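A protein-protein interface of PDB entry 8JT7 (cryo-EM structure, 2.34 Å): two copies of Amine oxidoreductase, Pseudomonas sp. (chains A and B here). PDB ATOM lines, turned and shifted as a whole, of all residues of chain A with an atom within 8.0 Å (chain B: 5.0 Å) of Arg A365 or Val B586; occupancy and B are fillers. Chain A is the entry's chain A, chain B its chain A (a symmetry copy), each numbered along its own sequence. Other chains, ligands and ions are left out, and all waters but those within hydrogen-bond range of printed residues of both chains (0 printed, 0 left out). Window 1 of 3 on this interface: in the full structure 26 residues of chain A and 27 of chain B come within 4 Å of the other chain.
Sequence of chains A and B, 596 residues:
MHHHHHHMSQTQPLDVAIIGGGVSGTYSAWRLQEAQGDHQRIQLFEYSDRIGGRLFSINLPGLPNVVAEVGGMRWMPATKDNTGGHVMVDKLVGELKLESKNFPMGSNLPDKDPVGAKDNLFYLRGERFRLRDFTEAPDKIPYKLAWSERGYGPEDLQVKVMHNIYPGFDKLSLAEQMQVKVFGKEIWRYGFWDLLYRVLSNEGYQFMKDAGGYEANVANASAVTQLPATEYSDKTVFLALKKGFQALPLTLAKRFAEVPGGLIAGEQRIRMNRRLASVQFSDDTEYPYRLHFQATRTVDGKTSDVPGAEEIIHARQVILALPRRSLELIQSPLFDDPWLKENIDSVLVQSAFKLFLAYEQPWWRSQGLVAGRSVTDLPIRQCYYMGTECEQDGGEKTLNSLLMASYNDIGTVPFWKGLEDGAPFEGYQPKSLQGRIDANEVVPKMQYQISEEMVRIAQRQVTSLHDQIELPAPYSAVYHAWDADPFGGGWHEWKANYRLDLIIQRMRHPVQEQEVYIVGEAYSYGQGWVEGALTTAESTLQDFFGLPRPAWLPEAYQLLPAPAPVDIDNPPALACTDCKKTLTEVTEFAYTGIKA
The guanidinium group (NH2) of Arg A365 lies within hydrogen-bond range of the backbone carbonyl oxygen (O) of Leu B583 (3.3 Å). OG1 of Thr B587 sits at hydrogen-bond distance from NE of Arg A365 (2.8 Å).
Printed residues of chain B within 4 Å of Arg A365: Leu B583, Thr B584, Val B586 and Thr B587. Printed residues of chain A within 4 Å of Val B586: Arg A365 (3.6 Å) and Ser A366 (3.4 Å). Printed residues of chain A within 4 Å of Glu B588: Leu A109 (3.1 Å). Printed residues of chain A within 4 Å of Leu B583: Arg A365 and Glu A391. Of the printed residues of chain B, Glu A391 touches Leu B583 (3.1 Å). Printed residues of chain B within 4 Å of Ser A366: His B163 (3.8 Å), Val B586 (3.4 Å) and Ala B590 (3.6 Å). Ser A107 touches none of the printed residues of chain B. The nearest residue of chain A that does not touch Val B586 is Gly A368 (5.6 Å).
OG of Ser A107 sits at hydrogen-bond distance from N of Leu A109 (3.3 Å). OE1 of Gln A361 sits close to N of Trp A363 (3.5 Å). The side-chain hydroxyl (OG) of Ser A366 sits at hydrogen-bond distance from the backbone carbonyl oxygen (O) of Trp A363 (3.0 Å). The side-chain carboxylate (OE2) of Glu A391 is in salt-bridge range of the guanidinium group (NH1) of Arg A365. ND1 of His B163 sits at hydrogen-bond distance from N of Gly B168, at 3.4 Å. The side-chain hydroxyl (OG1) of Thr B587 sits at hydrogen-bond distance from the backbone carbonyl oxygen (O) of Leu B583 (3.2 Å).
Hydrophobic or aromatic side chains of chain A within 4 Å of the printed part of chain B: Leu A109 and Val A370. Printed residues of chain B that touch a printed residue of chain A: His B163, Pro B167, Leu B583, Thr B584, Val B586, Thr B587, Glu B588 and Ala B590. Among the printed residues, 15 pairs touch across the chains. Among the printed residues, no Asp or Glu carboxylate lies within 4 Å of a Lys or Arg side-chain nitrogen of the other chain.
No position is printed for both chains. Of the 15 pairs that touch across the chains among the printed residues, none has its exchanged pair printed and touching as well.
CD2 of Leu A109 touches CG2 of Thr B584, 3.7 Å away. CG2 of Thr B587 touches CD1 of Leu A109, at 3.96 Å. OE2 of Glu B588 touches CB of Leu A109 (3.1 Å). Arg A365 touches Thr B584. CG1 of Val B586 touches C of Arg A365, 3.6 Å away. His B163 touches Ser A366. Ser A366 touches Val B586 (CA to CG1, 3.4 Å). O of Ser A366 touches CB of Ala B590, at 3.6 Å. CB of Ala B590 touches C of Gln A367 (3.7 Å). CG2 of Thr B587 touches CG2 of Val A370, at 3.5 Å.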
ATOM      1  N   SER A 107      30.681 -20.793  22.833  1.00  0.00           N
ATOM      2  CA  SER A 107      29.318 -20.400  22.524  1.00  0.00           C
ATOM      3  C   SER A 107      28.270 -21.265  23.236  1.00  0.00           C
ATOM      4  O   SER A 107      28.414 -22.477  23.327  1.00  0.00           O
ATOM      5  CB  SER A 107      29.120 -20.468  21.040  1.00  0.00           C
ATOM      6  OG  SER A 107      27.903 -19.831  20.645  1.00  0.00           O
ATOM      7  N   ASN A 108      27.160 -20.639  23.630  1.00  0.00           N
ATOM      8  CA  ASN A 108      26.050 -21.371  24.204  1.00  0.00           C
ATOM      9  C   ASN A 108      25.043 -21.695  23.097  1.00  0.00           C
ATOM     10  O   ASN A 108      24.277 -22.642  23.244  1.00  0.00           O
ATOM     11  CB  ASN A 108      25.483 -20.653  25.428  1.00  0.00           C
ATOM     12  CG  ASN A 108      25.340 -19.162  25.234  1.00  0.00           C
ATOM     13  OD1 ASN A 108      25.662 -18.626  24.169  1.00  0.00           O
ATOM     14  ND2 ASN A 108      24.902 -18.487  26.284  1.00  0.00           N
ATOM     15  N   LEU A 109      25.129 -20.992  21.963  1.00  0.00           N
ATOM     16  CA  LEU A 109      24.249 -21.211  20.825  1.00  0.00           C
ATOM     17  C   LEU A 109      24.798 -22.346  19.967  1.00  0.00           C
ATOM     18  O   LEU A 109      25.989 -22.661  20.040  1.00  0.00           O
ATOM     19  CB  LEU A 109      24.178 -19.940  19.980  1.00  0.00           C
ATOM     20  CG  LEU A 109      24.134 -18.636  20.778  1.00  0.00           C
ATOM     21  CD1 LEU A 109      24.532 -17.430  19.924  1.00  0.00           C
ATOM     22  CD2 LEU A 109      22.765 -18.461  21.414  1.00  0.00           C
ATOM     23  N   GLN A 361      31.052  -2.215  17.975  1.00  0.00           N
ATOM     24  CA  GLN A 361      30.226  -3.399  17.785  1.00  0.00           C
ATOM     25  C   GLN A 361      31.073  -4.657  17.913  1.00  0.00           C
ATOM     26  O   GLN A 361      32.272  -4.599  17.692  1.00  0.00           O
ATOM     27  CB  GLN A 361      29.509  -3.425  16.427  1.00  0.00           C
ATOM     28  CG  GLN A 361      30.387  -3.226  15.192  1.00  0.00           C
ATOM     29  CD  GLN A 361      30.260  -4.335  14.163  1.00  0.00           C
ATOM     30  OE1 GLN A 361      29.801  -5.438  14.438  1.00  0.00           O
ATOM     31  NE2 GLN A 361      30.760  -4.102  12.968  1.00  0.00           N
ATOM     32  N   PRO A 362      30.494  -5.825  18.274  1.00  0.00           N
ATOM     33  CA  PRO A 362      31.261  -7.067  18.320  1.00  0.00           C
ATOM     34  C   PRO A 362      31.381  -7.692  16.939  1.00  0.00           C
ATOM     35  O   PRO A 362      30.708  -8.672  16.652  1.00  0.00           O
ATOM     36  CB  PRO A 362      30.467  -7.959  19.270  1.00  0.00           C
ATOM     37  CG  PRO A 362      29.016  -7.467  19.102  1.00  0.00           C
ATOM     38  CD  PRO A 362      29.113  -6.002  18.755  1.00  0.00           C
ATOM     39  N   TRP A 363      32.294  -7.149  16.127  1.00  0.00           N
ATOM     40  CA  TRP A 363      32.489  -7.608  14.778  1.00  0.00           C
ATOM     41  C   TRP A 363      32.700  -9.131  14.730  1.00  0.00           C
ATOM     42  O   TRP A 363      32.465  -9.746  13.706  1.00  0.00           O
ATOM     43  CB  TRP A 363      33.578  -6.805  14.073  1.00  0.00           C
ATOM     44  CG  TRP A 363      34.832  -6.676  14.864  1.00  0.00           C
ATOM     45  CD1 TRP A 363      35.186  -5.614  15.623  1.00  0.00           C
ATOM     46  CD2 TRP A 363      35.867  -7.649  15.017  1.00  0.00           C
ATOM     47  NE1 TRP A 363      36.357  -5.862  16.270  1.00  0.00           N
ATOM     48  CE2 TRP A 363      36.802  -7.090  15.910  1.00  0.00           C
ATOM     49  CE3 TRP A 363      36.086  -8.939  14.523  1.00  0.00           C
ATOM     50  CZ2 TRP A 363      37.928  -7.776  16.318  1.00  0.00           C
ATOM     51  CZ3 TRP A 363      37.197  -9.631  14.952  1.00  0.00           C
ATOM     52  CH2 TRP A 363      38.086  -9.063  15.851  1.00  0.00           C
ATOM     53  N   TRP A 364      33.105  -9.753  15.831  1.00  0.00           N
ATOM     54  CA  TRP A 364      33.377 -11.177  15.802  1.00  0.00           C
ATOM     55  C   TRP A 364      32.113 -12.049  15.834  1.00  0.00           C
ATOM     56  O   TRP A 364      32.218 -13.227  15.521  1.00  0.00           O
ATOM     57  CB  TRP A 364      34.294 -11.553  16.965  1.00  0.00           C
ATOM     58  CG  TRP A 364      33.836 -11.040  18.280  1.00  0.00           C
ATOM     59  CD1 TRP A 364      32.977 -11.637  19.151  1.00  0.00           C
ATOM     60  CD2 TRP A 364      34.248  -9.806  18.884  1.00  0.00           C
ATOM     61  NE1 TRP A 364      32.820 -10.857  20.264  1.00  0.00           N
ATOM     62  CE2 TRP A 364      33.617  -9.742  20.139  1.00  0.00           C
ATOM     63  CE3 TRP A 364      35.129  -8.790  18.514  1.00  0.00           C
ATOM     64  CZ2 TRP A 364      33.851  -8.695  21.017  1.00  0.00           C
ATOM     65  CZ3 TRP A 364      35.284  -7.709  19.350  1.00  0.00           C
ATOM     66  CH2 TRP A 364      34.661  -7.672  20.590  1.00  0.00           C
ATOM     67  N   ARG A 365      30.969 -11.512  16.292  1.00  0.00           N
ATOM     68  CA  ARG A 365      29.731 -12.268  16.411  1.00  0.00           C
ATOM     69  C   ARG A 365      29.258 -12.685  15.026  1.00  0.00           C
ATOM     70  O   ARG A 365      28.856 -13.825  14.861  1.00  0.00           O
ATOM     71  CB  ARG A 365      28.632 -11.503  17.162  1.00  0.00           C
ATOM     72  CG  ARG A 365      28.990 -11.206  18.613  1.00  0.00           C
ATOM     73  CD  ARG A 365      29.076 -12.420  19.480  1.00  0.00           C
ATOM     74  NE  ARG A 365      27.851 -13.164  19.346  1.00  0.00           N
ATOM     75  CZ  ARG A 365      26.911 -13.267  20.261  1.00  0.00           C
ATOM     76  NH1 ARG A 365      27.014 -12.631  21.406  1.00  0.00           N
ATOM     77  NH2 ARG A 365      25.862 -14.025  20.015  1.00  0.00           N
ATOM     78  N   SER A 366      29.509 -11.838  14.028  1.00  0.00           N
ATOM     79  CA  SER A 366      29.196 -12.130  12.647  1.00  0.00           C
ATOM     80  C   SER A 366      30.189 -13.124  12.035  1.00  0.00           C
ATOM     81  O   SER A 366      30.032 -13.560  10.907  1.00  0.00           O
ATOM     82  CB  SER A 366      29.137 -10.829  11.882  1.00  0.00           C
ATOM     83  OG  SER A 366      30.440 -10.329  11.599  1.00  0.00           O
ATOM     84  N   GLN A 367      31.212 -13.531  12.774  1.00  0.00           N
ATOM     85  CA  GLN A 367      32.137 -14.529  12.255  1.00  0.00           C
ATOM     86  C   GLN A 367      31.899 -15.878  12.906  1.00  0.00           C
ATOM     87  O   GLN A 367      32.662 -16.806  12.690  1.00  0.00           O
ATOM     88  CB  GLN A 367      33.553 -14.021  12.528  1.00  0.00           C
ATOM     89  CG  GLN A 367      33.754 -12.595  12.000  1.00  0.00           C
ATOM     90  CD  GLN A 367      35.184 -12.134  11.850  1.00  0.00           C
ATOM     91  OE1 GLN A 367      36.136 -12.921  11.913  1.00  0.00           O
ATOM     92  NE2 GLN A 367      35.335 -10.849  11.560  1.00  0.00           N
ATOM     93  N   GLY A 368      30.878 -15.963  13.765  1.00  0.00           N
ATOM     94  CA  GLY A 368      30.629 -17.167  14.512  1.00  0.00           C
ATOM     95  C   GLY A 368      31.415 -17.234  15.815  1.00  0.00           C
ATOM     96  O   GLY A 368      31.528 -18.310  16.369  1.00  0.00           O
ATOM     97  N   LEU A 369      31.911 -16.111  16.338  1.00  0.00           N
ATOM     98  CA  LEU A 369      32.705 -16.159  17.557  1.00  0.00           C
ATOM     99  C   LEU A 369      31.963 -15.439  18.669  1.00  0.00           C
ATOM    100  O   LEU A 369      31.424 -14.351  18.454  1.00  0.00           O
ATOM    101  CB  LEU A 369      34.068 -15.509  17.288  1.00  0.00           C
ATOM    102  CG  LEU A 369      34.879 -16.232  16.217  1.00  0.00           C
ATOM    103  CD1 LEU A 369      35.931 -15.337  15.599  1.00  0.00           C
ATOM    104  CD2 LEU A 369      35.494 -17.467  16.807  1.00  0.00           C
ATOM    105  N   VAL A 370      31.969 -16.046  19.858  1.00  0.00           N
ATOM    106  CA  VAL A 370      31.150 -15.572  20.967  1.00  0.00           C
ATOM    107  C   VAL A 370      32.004 -15.378  22.206  1.00  0.00           C
ATOM    108  O   VAL A 370      32.003 -14.278  22.770  1.00  0.00           O
ATOM    109  CB  VAL A 370      29.978 -16.525  21.282  1.00  0.00           C
ATOM    110  CG1 VAL A 370      29.180 -16.013  22.446  1.00  0.00           C
ATOM    111  CG2 VAL A 370      29.071 -16.711  20.073  1.00  0.00           C
ATOM    112  N   ALA A 371      32.790 -16.379  22.595  1.00  0.00           N
ATOM    113  CA  ALA A 371      33.556 -16.272  23.826  1.00  0.00           C
ATOM    114  C   ALA A 371      34.745 -17.179  23.662  1.00  0.00           C
ATOM    115  O   ALA A 371      34.820 -17.917  22.682  1.00  0.00           O
ATOM    116  CB  ALA A 371      32.695 -16.691  25.024  1.00  0.00           C
ATOM    117  N   TYR A 385      37.327 -13.136  23.360  1.00  0.00           N
ATOM    118  CA  TYR A 385      36.148 -12.333  23.081  1.00  0.00           C
ATOM    119  C   TYR A 385      35.421 -12.052  24.372  1.00  0.00           C
ATOM    120  O   TYR A 385      34.883 -12.968  24.976  1.00  0.00           O
ATOM    121  CB  TYR A 385      35.273 -13.062  22.085  1.00  0.00           C
ATOM    122  CG  TYR A 385      36.073 -13.494  20.886  1.00  0.00           C
ATOM    123  CD1 TYR A 385      36.583 -12.566  19.987  1.00  0.00           C
ATOM    124  CD2 TYR A 385      36.418 -14.819  20.731  1.00  0.00           C
ATOM    125  CE1 TYR A 385      37.366 -12.966  18.918  1.00  0.00           C
ATOM    126  CE2 TYR A 385      37.240 -15.230  19.704  1.00  0.00           C
ATOM    127  CZ  TYR A 385      37.709 -14.297  18.797  1.00  0.00           C
ATOM    128  OH  TYR A 385      38.485 -14.786  17.801  1.00  0.00           O
ATOM    129  N   GLY A 387      32.812  -9.823  25.439  1.00  0.00           N
ATOM    130  CA  GLY A 387      31.503  -9.371  25.897  1.00  0.00           C
ATOM    131  C   GLY A 387      31.059  -7.989  25.434  1.00  0.00           C
ATOM    132  O   GLY A 387      31.857  -7.077  25.259  1.00  0.00           O
ATOM    133  N   THR A 388      29.747  -7.891  25.238  1.00  0.00           N
ATOM    134  CA  THR A 388      29.059  -6.731  24.698  1.00  0.00           C
ATOM    135  C   THR A 388      28.251  -6.138  25.838  1.00  0.00           C
ATOM    136  O   THR A 388      27.648  -6.887  26.594  1.00  0.00           O
ATOM    137  CB  THR A 388      28.224  -7.163  23.491  1.00  0.00           C
ATOM    138  OG1 THR A 388      29.186  -7.802  22.644  1.00  0.00           O
ATOM    139  CG2 THR A 388      27.481  -6.043  22.792  1.00  0.00           C
ATOM    140  N   CYS A 390      25.461  -4.505  25.958  1.00  0.00           N
ATOM    141  CA  CYS A 390      24.022  -4.721  25.899  1.00  0.00           C
ATOM    142  C   CYS A 390      23.622  -6.138  26.287  1.00  0.00           C
ATOM    143  O   CYS A 390      22.452  -6.366  26.563  1.00  0.00           O
ATOM    144  CB  CYS A 390      23.471  -4.432  24.504  1.00  0.00           C
ATOM    145  SG  CYS A 390      23.893  -5.663  23.241  1.00  0.00           S
ATOM    146  N   GLU A 391      24.549  -7.092  26.248  1.00  0.00           N
ATOM    147  CA  GLU A 391      24.233  -8.477  26.555  1.00  0.00           C
ATOM    148  C   GLU A 391      24.464  -8.768  28.027  1.00  0.00           C
ATOM    149  O   GLU A 391      24.318  -9.912  28.450  1.00  0.00           O
ATOM    150  CB  GLU A 391      25.115  -9.450  25.783  1.00  0.00           C
ATOM    151  CG  GLU A 391      24.812  -9.475  24.296  1.00  0.00           C
ATOM    152  CD  GLU A 391      25.026 -10.846  23.675  1.00  0.00           C
ATOM    153  OE1 GLU A 391      25.610 -11.721  24.360  1.00  0.00           O
ATOM    154  OE2 GLU A 391      24.565 -11.062  22.531  1.00  0.00           O
ATOM    155  N   LEU A 399      26.077  -1.557  21.712  1.00  0.00           N
ATOM    156  CA  LEU A 399      26.797  -2.707  21.179  1.00  0.00           C
ATOM    157  C   LEU A 399      28.291  -2.684  21.528  1.00  0.00           C
ATOM    158  O   LEU A 399      29.026  -3.491  20.976  1.00  0.00           O
ATOM    159  CB  LEU A 399      26.614  -2.700  19.661  1.00  0.00           C
ATOM    160  CG  LEU A 399      25.288  -3.226  19.147  1.00  0.00           C
ATOM    161  CD1 LEU A 399      25.207  -3.050  17.636  1.00  0.00           C
ATOM    162  CD2 LEU A 399      25.109  -4.674  19.540  1.00  0.00           C
ATOM    163  N   SER A 401      31.823  -3.376  22.744  1.00  0.00           N
ATOM    164  CA  SER A 401      32.343  -4.715  22.998  1.00  0.00           C
ATOM    165  C   SER A 401      33.836  -4.688  23.322  1.00  0.00           C
ATOM    166  O   SER A 401      34.556  -3.756  22.967  1.00  0.00           O
ATOM    167  CB  SER A 401      32.074  -5.580  21.818  1.00  0.00           C
ATOM    168  OG  SER A 401      30.676  -5.805  21.650  1.00  0.00           O
ATOM    169  N   HIS B 163      26.081  -8.164   8.016  1.00  0.00           N
ATOM    170  CA  HIS B 163      26.240  -8.269   9.463  1.00  0.00           C
ATOM    171  C   HIS B 163      27.646  -7.884   9.909  1.00  0.00           C
ATOM    172  O   HIS B 163      27.802  -7.289  10.959  1.00  0.00           O
ATOM    173  CB  HIS B 163      25.966  -9.685   9.933  1.00  0.00           C
ATOM    174  CG  HIS B 163      24.545 -10.065   9.820  1.00  0.00           C
ATOM    175  ND1 HIS B 163      23.529  -9.194  10.154  1.00  0.00           N
ATOM    176  CD2 HIS B 163      23.970 -11.218   9.460  1.00  0.00           C
ATOM    177  CE1 HIS B 163      22.383  -9.803   9.961  1.00  0.00           C
ATOM    178  NE2 HIS B 163      22.622 -11.043   9.575  1.00  0.00           N
ATOM    179  N   PRO B 167      25.710  -5.337  12.650  1.00  0.00           N
ATOM    180  CA  PRO B 167      24.855  -6.485  12.918  1.00  0.00           C
ATOM    181  C   PRO B 167      23.397  -6.056  13.038  1.00  0.00           C
ATOM    182  O   PRO B 167      23.079  -5.117  13.757  1.00  0.00           O
ATOM    183  CB  PRO B 167      25.447  -7.063  14.201  1.00  0.00           C
ATOM    184  CG  PRO B 167      26.093  -5.894  14.871  1.00  0.00           C
ATOM    185  CD  PRO B 167      26.599  -5.018  13.755  1.00  0.00           C
ATOM    186  N   GLY B 168      22.525  -6.786  12.349  1.00  0.00           N
ATOM    187  CA  GLY B 168      21.106  -6.481  12.294  1.00  0.00           C
ATOM    188  C   GLY B 168      20.745  -5.266  11.437  1.00  0.00           C
ATOM    189  O   GLY B 168      19.736  -4.646  11.710  1.00  0.00           O
ATOM    190  N   THR B 582      19.325 -10.004  18.194  1.00  0.00           N
ATOM    191  CA  THR B 582      20.113  -9.658  17.022  1.00  0.00           C
ATOM    192  C   THR B 582      21.461 -10.397  17.006  1.00  0.00           C
ATOM    193  O   THR B 582      21.832 -10.969  15.981  1.00  0.00           O
ATOM    194  CB  THR B 582      20.331  -8.141  16.929  1.00  0.00           C
ATOM    195  OG1 THR B 582      19.046  -7.542  16.723  1.00  0.00           O
ATOM    196  CG2 THR B 582      21.278  -7.735  15.813  1.00  0.00           C
ATOM    197  N   LEU B 583      22.198 -10.379  18.130  1.00  0.00           N
ATOM    198  CA  LEU B 583      23.502 -11.026  18.171  1.00  0.00           C
ATOM    199  C   LEU B 583      23.369 -12.524  18.026  1.00  0.00           C
ATOM    200  O   LEU B 583      24.212 -13.145  17.356  1.00  0.00           O
ATOM    201  CB  LEU B 583      24.260 -10.635  19.430  1.00  0.00           C
ATOM    202  CG  LEU B 583      24.606  -9.136  19.473  1.00  0.00           C
ATOM    203  CD1 LEU B 583      25.488  -8.828  20.660  1.00  0.00           C
ATOM    204  CD2 LEU B 583      25.257  -8.659  18.175  1.00  0.00           C
ATOM    205  N   THR B 584      22.275 -13.086  18.538  1.00  0.00           N
ATOM    206  CA  THR B 584      22.076 -14.516  18.393  1.00  0.00           C
ATOM    207  C   THR B 584      21.847 -14.853  16.918  1.00  0.00           C
ATOM    208  O   THR B 584      22.457 -15.769  16.382  1.00  0.00           O
ATOM    209  CB  THR B 584      20.946 -15.002  19.302  1.00  0.00           C
ATOM    210  OG1 THR B 584      21.371 -14.731  20.638  1.00  0.00           O
ATOM    211  CG2 THR B 584      20.631 -16.475  19.132  1.00  0.00           C
ATOM    212  N   GLU B 585      21.020 -14.061  16.249  1.00  0.00           N
ATOM    213  CA  GLU B 585      20.688 -14.302  14.856  1.00  0.00           C
ATOM    214  C   GLU B 585      21.964 -14.258  13.999  1.00  0.00           C
ATOM    215  O   GLU B 585      22.184 -15.119  13.155  1.00  0.00           O
ATOM    216  CB  GLU B 585      19.635 -13.292  14.370  1.00  0.00           C
ATOM    217  CG  GLU B 585      19.775 -12.999  12.874  1.00  0.00           C
ATOM    218  CD  GLU B 585      18.771 -12.061  12.214  1.00  0.00           C
ATOM    219  OE1 GLU B 585      17.591 -12.495  12.005  1.00  0.00           O
ATOM    220  OE2 GLU B 585      19.178 -10.900  11.874  1.00  0.00           O
ATOM    221  N   VAL B 586      22.756 -13.210  14.194  1.00  0.00           N
ATOM    222  CA  VAL B 586      24.011 -12.986  13.504  1.00  0.00           C
ATOM    223  C   VAL B 586      24.986 -14.158  13.718  1.00  0.00           C
ATOM    224  O   VAL B 586      25.551 -14.673  12.756  1.00  0.00           O
ATOM    225  CB  VAL B 586      24.587 -11.644  14.003  1.00  0.00           C
ATOM    226  CG1 VAL B 586      26.078 -11.547  13.892  1.00  0.00           C
ATOM    227  CG2 VAL B 586      23.928 -10.473  13.313  1.00  0.00           C
ATOM    228  N   THR B 587      25.154 -14.628  14.951  1.00  0.00           N
ATOM    229  CA  THR B 587      26.078 -15.718  15.202  1.00  0.00           C
ATOM    230  C   THR B 587      25.574 -17.020  14.586  1.00  0.00           C
ATOM    231  O   THR B 587      26.392 -17.783  14.066  1.00  0.00           O
ATOM    232  CB  THR B 587      26.373 -15.835  16.705  1.00  0.00           C
ATOM    233  OG1 THR B 587      27.059 -14.643  17.080  1.00  0.00           O
ATOM    234  CG2 THR B 587      27.251 -17.006  17.080  1.00  0.00           C
ATOM    235  N   GLU B 588      24.262 -17.298  14.672  1.00  0.00           N
ATOM    236  CA  GLU B 588      23.724 -18.538  14.121  1.00  0.00           C
ATOM    237  C   GLU B 588      23.807 -18.505  12.595  1.00  0.00           C
ATOM    238  O   GLU B 588      23.983 -19.544  11.944  1.00  0.00           O
ATOM    239  CB  GLU B 588      22.249 -18.756  14.431  1.00  0.00           C
ATOM    240  CG  GLU B 588      21.851 -18.556  15.875  1.00  0.00           C
ATOM    241  CD  GLU B 588      22.100 -19.717  16.805  1.00  0.00           C
ATOM    242  OE1 GLU B 588      21.103 -20.244  17.347  1.00  0.00           O
ATOM    243  OE2 GLU B 588      23.289 -20.059  17.010  1.00  0.00           O
ATOM    244  N   PHE B 589      23.649 -17.306  12.009  1.00  0.00           N
ATOM    245  CA  PHE B 589      23.833 -17.197  10.575  1.00  0.00           C
ATOM    246  C   PHE B 589      25.270 -17.586  10.228  1.00  0.00           C
ATOM    247  O   PHE B 589      25.505 -18.244   9.227  1.00  0.00           O
ATOM    248  CB  PHE B 589      23.500 -15.805  10.051  1.00  0.00           C
ATOM    249  CG  PHE B 589      23.666 -15.704   8.560  1.00  0.00           C
ATOM    250  CD1 PHE B 589      22.696 -16.190   7.695  1.00  0.00           C
ATOM    251  CD2 PHE B 589      24.844 -15.189   8.028  1.00  0.00           C
ATOM    252  CE1 PHE B 589      22.907 -16.127   6.321  1.00  0.00           C
ATOM    253  CE2 PHE B 589      25.038 -15.110   6.660  1.00  0.00           C
ATOM    254  CZ  PHE B 589      24.080 -15.613   5.814  1.00  0.00           C
ATOM    255  N   ALA B 590      26.238 -17.142  11.028  1.00  0.00           N
ATOM    256  CA  ALA B 590      27.633 -17.457  10.769  1.00  0.00           C
ATOM    257  C   ALA B 590      27.845 -18.967  10.849  1.00  0.00           C
ATOM    258  O   ALA B 590      28.552 -19.527  10.023  1.00  0.00           O
ATOM    259  CB  ALA B 590      28.540 -16.730  11.720  1.00  0.00           C
